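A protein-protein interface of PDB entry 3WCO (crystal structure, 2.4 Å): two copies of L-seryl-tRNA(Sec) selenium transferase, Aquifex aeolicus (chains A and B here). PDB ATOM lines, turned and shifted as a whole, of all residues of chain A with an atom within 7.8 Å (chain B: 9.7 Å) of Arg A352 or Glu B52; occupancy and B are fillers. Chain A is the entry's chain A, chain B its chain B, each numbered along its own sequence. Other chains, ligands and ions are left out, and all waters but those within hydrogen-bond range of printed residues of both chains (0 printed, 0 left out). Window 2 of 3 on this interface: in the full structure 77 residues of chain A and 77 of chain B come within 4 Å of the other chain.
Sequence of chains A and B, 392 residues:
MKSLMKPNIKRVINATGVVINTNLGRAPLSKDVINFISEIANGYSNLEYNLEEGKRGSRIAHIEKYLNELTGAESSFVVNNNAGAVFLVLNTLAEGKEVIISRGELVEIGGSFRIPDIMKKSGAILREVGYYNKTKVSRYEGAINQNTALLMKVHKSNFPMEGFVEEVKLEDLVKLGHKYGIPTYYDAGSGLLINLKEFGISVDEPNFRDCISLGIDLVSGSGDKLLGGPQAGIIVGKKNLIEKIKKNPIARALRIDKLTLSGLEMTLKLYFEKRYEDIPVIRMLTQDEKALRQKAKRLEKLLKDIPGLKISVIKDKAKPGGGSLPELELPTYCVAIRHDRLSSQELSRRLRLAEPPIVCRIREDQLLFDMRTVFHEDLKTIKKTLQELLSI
Of the printed residues of chain B, Arg A352 touches Tyr B49, Leu B51, Glu B52, Glu B53 and Gly B54. Glu B52 touches one residue of chain A. Ser A348 touches none of the printed residues of chain B. Leu A353 touches just one residue of chain B: Leu B51. No residue of chain B comes within 4 Å of Ala A354. Of the printed residues of chain A, Leu B51 touches Lys A10 (3.98 Å), Arg A352 (2.7 Å), Leu A353 (3.96 Å) and Pro A357 (3.97 Å). Of the printed residues of chain A, Glu B53 touches Arg A352. The nearest residue of chain B that does not touch Arg A352 is Asn B50 (4.9 Å).
No position is printed for both chains.
O of Asn B46 is in hydrogen-bond range of NE2 of His B62, 2.9 Å away. The side-chain hydroxyl (OH) of Tyr B49 is in hydrogen-bond range of the backbone carbonyl oxygen (O) of Gly B54, 3.2 Å away. The side-chain amide oxygen (OD1) of Asn B50 lies close to the side-chain carboxylate (OE1) of Glu B52 (2.8 Å). The side-chain amide oxygen of Asn B50 lies within hydrogen-bond range of the backbone NH of Glu B53 (3.1 Å).
Hydrophobic or aromatic side chains of chain A within 4 Å of the printed part of chain B: Leu A353, Pro A357 and Val A359. Along chain A the printed residues that touch a printed residue of chain B span positions 8 to 359. Printed residues of chain B that touch a printed residue of chain A: Asn B46, Tyr B49, Leu B51, Glu B52, Glu B53, Gly B54 and His B62. Hydrophobic or aromatic side chains of chain B that line the printed part of chain A: Tyr B49, Leu B51 and His B62. Among the printed residues, 12 pairs touch across the chains. Among the printed residues, no Asp or Glu carboxylate lies within 4 Å of a Lys or Arg side-chain nitrogen of the other chain.
Lys A10 touches Leu B51. CD of Arg A352 touches OH of Tyr B49 (3.8 Å). Arg A352 touches Glu B53. Leu B51 touches Leu A353. Pro A357 touches Leu B51 (CG to CD1, 3.97 Å). Tyr B49 touches Val A359.
ND2 of Asn B46 lies within hydrogen-bond range of O of Asn A8 (2.8 Å). ND2 of Asn A8 sits at hydrogen-bond distance from O of His B62 (2.9 Å). The backbone NH of Lys A10 sits at hydrogen-bond distance from the side-chain amide oxygen of Asn B46, 2.7 Å away. The guanidinium group (NE) of Arg A352 lies within hydrogen-bond range of the backbone carbonyl oxygen (O) of Leu B51, 2.7 Å away. O of Glu B52 sits at hydrogen-bond distance from NH2 of Arg A352 (3.0 Å). The guanidinium group (NH2) of Arg A352 lies close to the backbone NH (N) of Gly B54 (3.4 Å).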
ATOM      1  N   LYS A   6       9.614   0.518  12.593  1.00  0.00           N
ATOM      2  CA  LYS A   6       8.484   1.290  13.105  1.00  0.00           C
ATOM      3  C   LYS A   6       7.244   0.386  13.236  1.00  0.00           C
ATOM      4  O   LYS A   6       7.030  -0.503  12.414  1.00  0.00           O
ATOM      5  CB  LYS A   6       8.211   2.509  12.207  1.00  0.00           C
ATOM      6  CG  LYS A   6       8.389   2.226  10.720  1.00  0.00           C
ATOM      7  CD  LYS A   6       7.411   3.025   9.843  1.00  0.00           C
ATOM      8  CE  LYS A   6       7.322   2.428   8.425  1.00  0.00           C
ATOM      9  NZ  LYS A   6       6.378   3.170   7.535  1.00  0.00           N
ATOM     10  N   ASN A   8       3.383  -1.028  13.078  1.00  0.00           N
ATOM     11  CA  ASN A   8       2.371  -0.859  12.030  1.00  0.00           C
ATOM     12  C   ASN A   8       1.200   0.037  12.454  1.00  0.00           C
ATOM     13  O   ASN A   8       0.587   0.727  11.638  1.00  0.00           O
ATOM     14  CB  ASN A   8       1.833  -2.211  11.590  1.00  0.00           C
ATOM     15  CG  ASN A   8       2.918  -3.126  11.060  1.00  0.00           C
ATOM     16  OD1 ASN A   8       3.746  -2.723  10.235  1.00  0.00           O
ATOM     17  ND2 ASN A   8       2.925  -4.371  11.541  1.00  0.00           N
ATOM     18  N   LYS A  10      -0.208   3.275  13.941  1.00  0.00           N
ATOM     19  CA  LYS A  10       0.426   4.578  14.103  1.00  0.00           C
ATOM     20  C   LYS A  10      -0.561   5.712  14.267  1.00  0.00           C
ATOM     21  O   LYS A  10      -1.708   5.612  13.843  1.00  0.00           O
ATOM     22  CB  LYS A  10       1.371   4.854  12.931  1.00  0.00           C
ATOM     23  CG  LYS A  10       0.680   4.933  11.608  1.00  0.00           C
ATOM     24  CD  LYS A  10       1.707   4.857  10.467  1.00  0.00           C
ATOM     25  CE  LYS A  10       2.406   3.522  10.464  1.00  0.00           C
ATOM     26  NZ  LYS A  10       3.392   3.432   9.380  1.00  0.00           N
ATOM     27  N   VAL A  12      -2.339   9.169  13.430  1.00  0.00           N
ATOM     28  CA  VAL A  12      -2.660   9.773  12.145  1.00  0.00           C
ATOM     29  C   VAL A  12      -3.387  11.094  12.365  1.00  0.00           C
ATOM     30  O   VAL A  12      -4.265  11.179  13.212  1.00  0.00           O
ATOM     31  CB  VAL A  12      -3.597   8.850  11.352  1.00  0.00           C
ATOM     32  CG1 VAL A  12      -4.414   9.640  10.356  1.00  0.00           C
ATOM     33  CG2 VAL A  12      -2.817   7.750  10.666  1.00  0.00           C
ATOM     34  N   SER A 344      -5.328  15.409  -7.036  1.00  0.00           N
ATOM     35  CA  SER A 344      -5.785  15.171  -5.673  1.00  0.00           C
ATOM     36  C   SER A 344      -5.566  13.738  -5.207  1.00  0.00           C
ATOM     37  O   SER A 344      -5.138  13.524  -4.077  1.00  0.00           O
ATOM     38  CB  SER A 344      -7.258  15.546  -5.539  1.00  0.00           C
ATOM     39  OG  SER A 344      -7.436  16.934  -5.747  1.00  0.00           O
ATOM     40  N   GLN A 345      -5.865  12.765  -6.066  1.00  0.00           N
ATOM     41  CA  GLN A 345      -5.643  11.362  -5.721  1.00  0.00           C
ATOM     42  C   GLN A 345      -4.199  11.127  -5.308  1.00  0.00           C
ATOM     43  O   GLN A 345      -3.929  10.639  -4.204  1.00  0.00           O
ATOM     44  CB  GLN A 345      -6.001  10.427  -6.883  1.00  0.00           C
ATOM     45  CG  GLN A 345      -7.478  10.412  -7.266  1.00  0.00           C
ATOM     46  CD  GLN A 345      -8.411  10.082  -6.106  1.00  0.00           C
ATOM     47  OE1 GLN A 345      -8.020   9.437  -5.127  1.00  0.00           O
ATOM     48  NE2 GLN A 345      -9.663  10.526  -6.219  1.00  0.00           N
ATOM     49  N   GLU A 346      -3.279  11.495  -6.195  1.00  0.00           N
ATOM     50  CA  GLU A 346      -1.859  11.306  -5.950  1.00  0.00           C
ATOM     51  C   GLU A 346      -1.371  12.085  -4.740  1.00  0.00           C
ATOM     52  O   GLU A 346      -0.556  11.577  -3.959  1.00  0.00           O
ATOM     53  CB  GLU A 346      -1.046  11.700  -7.179  1.00  0.00           C
ATOM     54  CG  GLU A 346       0.457  11.541  -6.988  1.00  0.00           C
ATOM     55  CD  GLU A 346       0.863  10.125  -6.606  1.00  0.00           C
ATOM     56  OE1 GLU A 346       0.125   9.169  -6.931  1.00  0.00           O
ATOM     57  OE2 GLU A 346       1.933   9.966  -5.979  1.00  0.00           O
ATOM     58  N   LEU A 347      -1.867  13.311  -4.586  1.00  0.00           N
ATOM     59  CA  LEU A 347      -1.517  14.112  -3.424  1.00  0.00           C
ATOM     60  C   LEU A 347      -2.014  13.423  -2.151  1.00  0.00           C
ATOM     61  O   LEU A 347      -1.246  13.235  -1.196  1.00  0.00           O
ATOM     62  CB  LEU A 347      -2.086  15.524  -3.545  1.00  0.00           C
ATOM     63  CG  LEU A 347      -1.668  16.484  -2.434  1.00  0.00           C
ATOM     64  CD1 LEU A 347      -0.169  16.378  -2.178  1.00  0.00           C
ATOM     65  CD2 LEU A 347      -2.064  17.915  -2.784  1.00  0.00           C
ATOM     66  N   SER A 348      -3.287  13.029  -2.162  1.00  0.00           N
ATOM     67  CA  SER A 348      -3.874  12.222  -1.095  1.00  0.00           C
ATOM     68  C   SER A 348      -2.999  11.040  -0.738  1.00  0.00           C
ATOM     69  O   SER A 348      -2.707  10.827   0.441  1.00  0.00           O
ATOM     70  CB  SER A 348      -5.247  11.697  -1.518  1.00  0.00           C
ATOM     71  OG  SER A 348      -6.280  12.379  -0.840  1.00  0.00           O
ATOM     72  N   ARG A 349      -2.590  10.264  -1.743  1.00  0.00           N
ATOM     73  CA  ARG A 349      -1.773   9.081  -1.475  1.00  0.00           C
ATOM     74  C   ARG A 349      -0.500   9.456  -0.727  1.00  0.00           C
ATOM     75  O   ARG A 349      -0.129   8.790   0.243  1.00  0.00           O
ATOM     76  CB  ARG A 349      -1.424   8.313  -2.755  1.00  0.00           C
ATOM     77  CG  ARG A 349      -0.766   6.955  -2.471  1.00  0.00           C
ATOM     78  CD  ARG A 349      -0.185   6.306  -3.731  1.00  0.00           C
ATOM     79  NE  ARG A 349       0.914   7.088  -4.298  1.00  0.00           N
ATOM     80  CZ  ARG A 349       2.195   6.917  -3.978  1.00  0.00           C
ATOM     81  NH1 ARG A 349       2.542   5.982  -3.094  1.00  0.00           N
ATOM     82  NH2 ARG A 349       3.130   7.676  -4.541  1.00  0.00           N
ATOM     83  N   ARG A 350       0.148  10.535  -1.165  1.00  0.00           N
ATOM     84  CA  ARG A 350       1.386  10.976  -0.533  1.00  0.00           C
ATOM     85  C   ARG A 350       1.206  11.441   0.918  1.00  0.00           C
ATOM     86  O   ARG A 350       2.082  11.210   1.757  1.00  0.00           O
ATOM     87  CB  ARG A 350       2.053  12.052  -1.380  1.00  0.00           C
ATOM     88  CG  ARG A 350       2.356  11.562  -2.786  1.00  0.00           C
ATOM     89  CD  ARG A 350       3.335  12.455  -3.499  1.00  0.00           C
ATOM     90  NE  ARG A 350       3.630  11.947  -4.833  1.00  0.00           N
ATOM     91  CZ  ARG A 350       4.560  12.458  -5.630  1.00  0.00           C
ATOM     92  NH1 ARG A 350       5.282  13.486  -5.217  1.00  0.00           N
ATOM     93  NH2 ARG A 350       4.767  11.945  -6.834  1.00  0.00           N
ATOM     94  N   LEU A 351       0.075  12.082   1.207  1.00  0.00           N
ATOM     95  CA  LEU A 351      -0.237  12.519   2.569  1.00  0.00           C
ATOM     96  C   LEU A 351      -0.346  11.307   3.500  1.00  0.00           C
ATOM     97  O   LEU A 351       0.165  11.317   4.620  1.00  0.00           O
ATOM     98  CB  LEU A 351      -1.526  13.367   2.592  1.00  0.00           C
ATOM     99  CG  LEU A 351      -1.415  14.734   1.897  1.00  0.00           C
ATOM    100  CD1 LEU A 351      -2.754  15.445   1.783  1.00  0.00           C
ATOM    101  CD2 LEU A 351      -0.418  15.613   2.610  1.00  0.00           C
ATOM    102  N   ARG A 352      -0.972  10.243   3.009  1.00  0.00           N
ATOM    103  CA  ARG A 352      -1.121   9.028   3.792  1.00  0.00           C
ATOM    104  C   ARG A 352       0.199   8.325   4.136  1.00  0.00           C
ATOM    105  O   ARG A 352       0.256   7.530   5.083  1.00  0.00           O
ATOM    106  CB  ARG A 352      -2.100   8.080   3.095  1.00  0.00           C
ATOM    107  CG  ARG A 352      -3.457   8.726   2.882  1.00  0.00           C
ATOM    108  CD  ARG A 352      -4.534   7.718   2.516  1.00  0.00           C
ATOM    109  NE  ARG A 352      -4.132   6.820   1.438  1.00  0.00           N
ATOM    110  CZ  ARG A 352      -4.382   7.028   0.149  1.00  0.00           C
ATOM    111  NH1 ARG A 352      -5.032   8.126  -0.238  1.00  0.00           N
ATOM    112  NH2 ARG A 352      -3.984   6.131  -0.753  1.00  0.00           N
ATOM    113  N   LEU A 353       1.261   8.626   3.394  1.00  0.00           N
ATOM    114  CA  LEU A 353       2.545   7.964   3.629  1.00  0.00           C
ATOM    115  C   LEU A 353       3.523   8.837   4.423  1.00  0.00           C
ATOM    116  O   LEU A 353       4.596   8.381   4.818  1.00  0.00           O
ATOM    117  CB  LEU A 353       3.160   7.492   2.310  1.00  0.00           C
ATOM    118  CG  LEU A 353       2.212   6.768   1.346  1.00  0.00           C
ATOM    119  CD1 LEU A 353       2.956   6.251   0.114  1.00  0.00           C
ATOM    120  CD2 LEU A 353       1.477   5.635   2.030  1.00  0.00           C
ATOM    121  N   ALA A 354       3.127  10.083   4.678  1.00  0.00           N
ATOM    122  CA  ALA A 354       3.920  11.007   5.491  1.00  0.00           C
ATOM    123  C   ALA A 354       4.067  10.550   6.948  1.00  0.00           C
ATOM    124  O   ALA A 354       3.410   9.600   7.392  1.00  0.00           O
ATOM    125  CB  ALA A 354       3.306  12.395   5.442  1.00  0.00           C
ATOM    126  N   GLU A 355       4.944  11.232   7.680  1.00  0.00           N
ATOM    127  CA  GLU A 355       5.162  10.956   9.093  1.00  0.00           C
ATOM    128  C   GLU A 355       5.027  12.254   9.858  1.00  0.00           C
ATOM    129  O   GLU A 355       5.925  13.093   9.814  1.00  0.00           O
ATOM    130  CB  GLU A 355       6.558  10.392   9.329  1.00  0.00           C
ATOM    131  CG  GLU A 355       6.883   9.160   8.514  1.00  0.00           C
ATOM    132  CD  GLU A 355       8.376   8.890   8.462  1.00  0.00           C
ATOM    133  OE1 GLU A 355       9.142   9.700   9.029  1.00  0.00           O
ATOM    134  OE2 GLU A 355       8.782   7.876   7.854  1.00  0.00           O
ATOM    135  N   PRO A 356       3.902  12.433  10.559  1.00  0.00           N
ATOM    136  CA  PRO A 356       2.779  11.489  10.656  1.00  0.00           C
ATOM    137  C   PRO A 356       1.828  11.568   9.461  1.00  0.00           C
ATOM    138  O   PRO A 356       1.758  12.610   8.796  1.00  0.00           O
ATOM    139  CB  PRO A 356       2.055  11.958  11.916  1.00  0.00           C
ATOM    140  CG  PRO A 356       2.312  13.450  11.941  1.00  0.00           C
ATOM    141  CD  PRO A 356       3.706  13.625  11.405  1.00  0.00           C
ATOM    142  N   PRO A 357       1.100  10.471   9.195  1.00  0.00           N
ATOM    143  CA  PRO A 357       0.166  10.409   8.061  1.00  0.00           C
ATOM    144  C   PRO A 357      -0.975  11.404   8.217  1.00  0.00           C
ATOM    145  O   PRO A 357      -1.386  11.708   9.343  1.00  0.00           O
ATOM    146  CB  PRO A 357      -0.409   8.991   8.150  1.00  0.00           C
ATOM    147  CG  PRO A 357       0.578   8.211   9.001  1.00  0.00           C
ATOM    148  CD  PRO A 357       1.129   9.215   9.964  1.00  0.00           C
ATOM    149  N   ILE A 358      -1.490  11.886   7.093  1.00  0.00           N
ATOM    150  CA  ILE A 358      -2.592  12.835   7.094  1.00  0.00           C
ATOM    151  C   ILE A 358      -3.703  12.288   6.207  1.00  0.00           C
ATOM    152  O   ILE A 358      -3.446  11.804   5.102  1.00  0.00           O
ATOM    153  CB  ILE A 358      -2.133  14.206   6.571  1.00  0.00           C
ATOM    154  CG1 ILE A 358      -0.938  14.704   7.398  1.00  0.00           C
ATOM    155  CG2 ILE A 358      -3.271  15.200   6.630  1.00  0.00           C
ATOM    156  CD1 ILE A 358      -0.325  15.985   6.901  1.00  0.00           C
ATOM    157  N   VAL A 359      -4.935  12.342   6.693  1.00  0.00           N
ATOM    158  CA  VAL A 359      -6.040  11.718   5.985  1.00  0.00           C
ATOM    159  C   VAL A 359      -7.124  12.759   5.738  1.00  0.00           C
ATOM    160  O   VAL A 359      -7.876  13.109   6.657  1.00  0.00           O
ATOM    161  CB  VAL A 359      -6.621  10.527   6.780  1.00  0.00           C
ATOM    162  CG1 VAL A 359      -7.760   9.844   5.999  1.00  0.00           C
ATOM    163  CG2 VAL A 359      -5.542   9.532   7.086  1.00  0.00           C
ATOM    164  N   CYS A 360      -7.196  13.268   4.509  1.00  0.00           N
ATOM    165  CA  CYS A 360      -8.208  14.265   4.179  1.00  0.00           C
ATOM    166  C   CYS A 360      -9.362  13.580   3.465  1.00  0.00           C
ATOM    167  O   CYS A 360      -9.326  12.364   3.241  1.00  0.00           O
ATOM    168  CB  CYS A 360      -7.608  15.369   3.306  1.00  0.00           C
ATOM    169  SG  CYS A 360      -6.825  14.774   1.794  1.00  0.00           S
ATOM    170  N   ILE A 362     -11.864  13.950  -0.168  1.00  0.00           N
ATOM    171  CA  ILE A 362     -11.808  14.531  -1.502  1.00  0.00           C
ATOM    172  C   ILE A 362     -13.215  14.859  -2.002  1.00  0.00           C
ATOM    173  O   ILE A 362     -14.170  14.119  -1.743  1.00  0.00           O
ATOM    174  CB  ILE A 362     -11.086  13.589  -2.495  1.00  0.00           C
ATOM    175  CG1 ILE A 362      -9.733  13.163  -1.924  1.00  0.00           C
ATOM    176  CG2 ILE A 362     -10.895  14.252  -3.846  1.00  0.00           C
ATOM    177  CD1 ILE A 362      -8.786  12.579  -2.954  1.00  0.00           C
ATOM    178  N   THR A 385       4.394  19.334   5.999  1.00  0.00           N
ATOM    179  CA  THR A 385       4.312  18.133   5.176  1.00  0.00           C
ATOM    180  C   THR A 385       3.970  18.461   3.720  1.00  0.00           C
ATOM    181  O   THR A 385       4.523  17.868   2.792  1.00  0.00           O
ATOM    182  CB  THR A 385       3.267  17.148   5.749  1.00  0.00           C
ATOM    183  OG1 THR A 385       3.750  16.591   6.979  1.00  0.00           O
ATOM    184  CG2 THR A 385       2.974  16.024   4.767  1.00  0.00           C
ATOM    185  N   LEU A 389       6.217  17.655   0.208  1.00  0.00           N
ATOM    186  CA  LEU A 389       5.620  16.946  -0.916  1.00  0.00           C
ATOM    187  C   LEU A 389       5.451  17.822  -2.166  1.00  0.00           C
ATOM    188  O   LEU A 389       5.171  17.314  -3.252  1.00  0.00           O
ATOM    189  CB  LEU A 389       4.272  16.350  -0.497  1.00  0.00           C
ATOM    190  CG  LEU A 389       4.385  15.313   0.618  1.00  0.00           C
ATOM    191  CD1 LEU A 389       3.052  14.663   0.927  1.00  0.00           C
ATOM    192  CD2 LEU A 389       5.409  14.267   0.226  1.00  0.00           C
ATOM    193  N   ASN B  46      -4.497   4.486  12.508  1.00  0.00           N
ATOM    194  CA  ASN B  46      -4.780   3.699  11.316  1.00  0.00           C
ATOM    195  C   ASN B  46      -5.318   2.333  11.727  1.00  0.00           C
ATOM    196  O   ASN B  46      -5.119   1.343  11.022  1.00  0.00           O
ATOM    197  CB  ASN B  46      -3.504   3.552  10.471  1.00  0.00           C
ATOM    198  CG  ASN B  46      -2.404   2.714  11.172  1.00  0.00           C
ATOM    199  OD1 ASN B  46      -2.357   2.609  12.404  1.00  0.00           O
ATOM    200  ND2 ASN B  46      -1.512   2.131  10.374  1.00  0.00           N
ATOM    201  N   TYR B  49      -7.499   1.004   9.065  1.00  0.00           N
ATOM    202  CA  TYR B  49      -7.249   1.759   7.847  1.00  0.00           C
ATOM    203  C   TYR B  49      -5.975   1.339   7.131  1.00  0.00           C
ATOM    204  O   TYR B  49      -4.892   1.340   7.720  1.00  0.00           O
ATOM    205  CB  TYR B  49      -7.163   3.241   8.182  1.00  0.00           C
ATOM    206  CG  TYR B  49      -7.378   4.149   6.999  1.00  0.00           C
ATOM    207  CD1 TYR B  49      -6.433   5.100   6.654  1.00  0.00           C
ATOM    208  CD2 TYR B  49      -8.528   4.062   6.224  1.00  0.00           C
ATOM    209  CE1 TYR B  49      -6.625   5.956   5.579  1.00  0.00           C
ATOM    210  CE2 TYR B  49      -8.731   4.918   5.136  1.00  0.00           C
ATOM    211  CZ  TYR B  49      -7.772   5.862   4.827  1.00  0.00           C
ATOM    212  OH  TYR B  49      -7.948   6.708   3.767  1.00  0.00           O
ATOM    213  N   ASN B  50      -6.105   0.993   5.855  1.00  0.00           N
ATOM    214  CA  ASN B  50      -4.947   0.717   5.016  1.00  0.00           C
ATOM    215  C   ASN B  50      -4.449   2.003   4.342  1.00  0.00           C
ATOM    216  O   ASN B  50      -4.985   2.419   3.318  1.00  0.00           O
ATOM    217  CB  ASN B  50      -5.323  -0.325   3.966  1.00  0.00           C
ATOM    218  CG  ASN B  50      -4.155  -0.702   3.046  1.00  0.00           C
ATOM    219  OD1 ASN B  50      -3.251   0.095   2.778  1.00  0.00           O
ATOM    220  ND2 ASN B  50      -4.197  -1.926   2.537  1.00  0.00           N
ATOM    221  N   LEU B  51      -3.396   2.598   4.896  1.00  0.00           N
ATOM    222  CA  LEU B  51      -2.863   3.876   4.415  1.00  0.00           C
ATOM    223  C   LEU B  51      -2.325   3.900   2.983  1.00  0.00           C
ATOM    224  O   LEU B  51      -2.413   4.920   2.298  1.00  0.00           O
ATOM    225  CB  LEU B  51      -1.774   4.347   5.363  1.00  0.00           C
ATOM    226  CG  LEU B  51      -2.310   4.792   6.717  1.00  0.00           C
ATOM    227  CD1 LEU B  51      -1.191   4.887   7.739  1.00  0.00           C
ATOM    228  CD2 LEU B  51      -3.005   6.127   6.543  1.00  0.00           C
ATOM    229  N   GLU B  52      -1.758   2.789   2.532  1.00  0.00           N
ATOM    230  CA  GLU B  52      -1.209   2.727   1.181  1.00  0.00           C
ATOM    231  C   GLU B  52      -2.351   2.819   0.187  1.00  0.00           C
ATOM    232  O   GLU B  52      -2.314   3.628  -0.736  1.00  0.00           O
ATOM    233  CB  GLU B  52      -0.396   1.442   0.974  1.00  0.00           C
ATOM    234  CG  GLU B  52       0.836   1.316   1.899  1.00  0.00           C
ATOM    235  CD  GLU B  52       0.489   1.174   3.392  1.00  0.00           C
ATOM    236  OE1 GLU B  52      -0.677   0.859   3.723  1.00  0.00           O
ATOM    237  OE2 GLU B  52       1.382   1.382   4.243  1.00  0.00           O
ATOM    238  N   GLU B  53      -3.391   2.023   0.416  1.00  0.00           N
ATOM    239  CA  GLU B  53      -4.551   2.014  -0.463  1.00  0.00           C
ATOM    240  C   GLU B  53      -5.622   3.054  -0.090  1.00  0.00           C
ATOM    241  O   GLU B  53      -6.572   3.264  -0.841  1.00  0.00           O
ATOM    242  CB  GLU B  53      -5.147   0.610  -0.495  1.00  0.00           C
ATOM    243  CG  GLU B  53      -4.162  -0.433  -0.976  1.00  0.00           C
ATOM    244  CD  GLU B  53      -3.597  -0.097  -2.345  1.00  0.00           C
ATOM    245  OE1 GLU B  53      -4.386   0.308  -3.228  1.00  0.00           O
ATOM    246  OE2 GLU B  53      -2.368  -0.227  -2.538  1.00  0.00           O
ATOM    247  N   GLY B  54      -5.450   3.711   1.057  1.00  0.00           N
ATOM    248  CA  GLY B  54      -6.394   4.717   1.533  1.00  0.00           C
ATOM    249  C   GLY B  54      -7.822   4.230   1.668  1.00  0.00           C
ATOM    250  O   GLY B  54      -8.764   4.899   1.260  1.00  0.00           O
ATOM    251  N   LYS B  55      -7.979   3.059   2.262  1.00  0.00           N
ATOM    252  CA  LYS B  55      -9.263   2.384   2.292  1.00  0.00           C
ATOM    253  C   LYS B  55      -9.340   1.633   3.610  1.00  0.00           C
ATOM    254  O   LYS B  55      -8.315   1.428   4.269  1.00  0.00           O
ATOM    255  CB  LYS B  55      -9.336   1.408   1.116  1.00  0.00           C
ATOM    256  CG  LYS B  55     -10.735   1.066   0.637  1.00  0.00           C
ATOM    257  CD  LYS B  55     -10.669   0.340  -0.709  1.00  0.00           C
ATOM    258  CE  LYS B  55     -12.060  -0.005  -1.224  1.00  0.00           C
ATOM    259  NZ  LYS B  55     -12.061  -0.407  -2.657  1.00  0.00           N
ATOM    260  N   ARG B  56     -10.544   1.230   4.005  1.00  0.00           N
ATOM    261  CA  ARG B  56     -10.700   0.380   5.181  1.00  0.00           C
ATOM    262  C   ARG B  56      -9.807  -0.870   5.108  1.00  0.00           C
ATOM    263  O   ARG B  56      -9.596  -1.423   4.028  1.00  0.00           O
ATOM    264  CB  ARG B  56     -12.160  -0.041   5.355  1.00  0.00           C
ATOM    265  CG  ARG B  56     -12.366  -0.810   6.638  1.00  0.00           C
ATOM    266  CD  ARG B  56     -13.749  -1.351   6.833  1.00  0.00           C
ATOM    267  NE  ARG B  56     -13.665  -2.465   7.772  1.00  0.00           N
ATOM    268  CZ  ARG B  56     -14.697  -3.065   8.352  1.00  0.00           C
ATOM    269  NH1 ARG B  56     -15.941  -2.664   8.110  1.00  0.00           N
ATOM    270  NH2 ARG B  56     -14.471  -4.074   9.187  1.00  0.00           N
ATOM    271  N   GLY B  57      -9.268  -1.296   6.248  1.00  0.00           N
ATOM    272  CA  GLY B  57      -8.487  -2.521   6.311  1.00  0.00           C
ATOM    273  C   GLY B  57      -8.712  -3.221   7.637  1.00  0.00           C
ATOM    274  O   GLY B  57      -9.218  -2.611   8.574  1.00  0.00           O
ATOM    275  N   ALA B  61      -4.261  -7.250  10.515  1.00  0.00           N
ATOM    276  CA  ALA B  61      -3.102  -7.116   9.647  1.00  0.00           C
ATOM    277  C   ALA B  61      -1.943  -6.411  10.347  1.00  0.00           C
ATOM    278  O   ALA B  61      -0.815  -6.492   9.899  1.00  0.00           O
ATOM    279  CB  ALA B  61      -3.476  -6.386   8.379  1.00  0.00           C
ATOM    280  N   HIS B  62      -2.223  -5.711  11.436  1.00  0.00           N
ATOM    281  CA  HIS B  62      -1.192  -4.943  12.127  1.00  0.00           C
ATOM    282  C   HIS B  62      -0.246  -5.818  12.955  1.00  0.00           C
ATOM    283  O   HIS B  62       0.855  -5.386  13.303  1.00  0.00           O
ATOM    284  CB  HIS B  62      -1.829  -3.894  13.043  1.00  0.00           C
ATOM    285  CG  HIS B  62      -2.433  -2.736  12.314  1.00  0.00           C
ATOM    286  ND1 HIS B  62      -1.679  -1.846  11.583  1.00  0.00           N
ATOM    287  CD2 HIS B  62      -3.715  -2.310  12.223  1.00  0.00           C
ATOM    288  CE1 HIS B  62      -2.475  -0.931  11.052  1.00  0.00           C
ATOM    289  NE2 HIS B  62      -3.713  -1.189  11.429  1.00  0.00           N
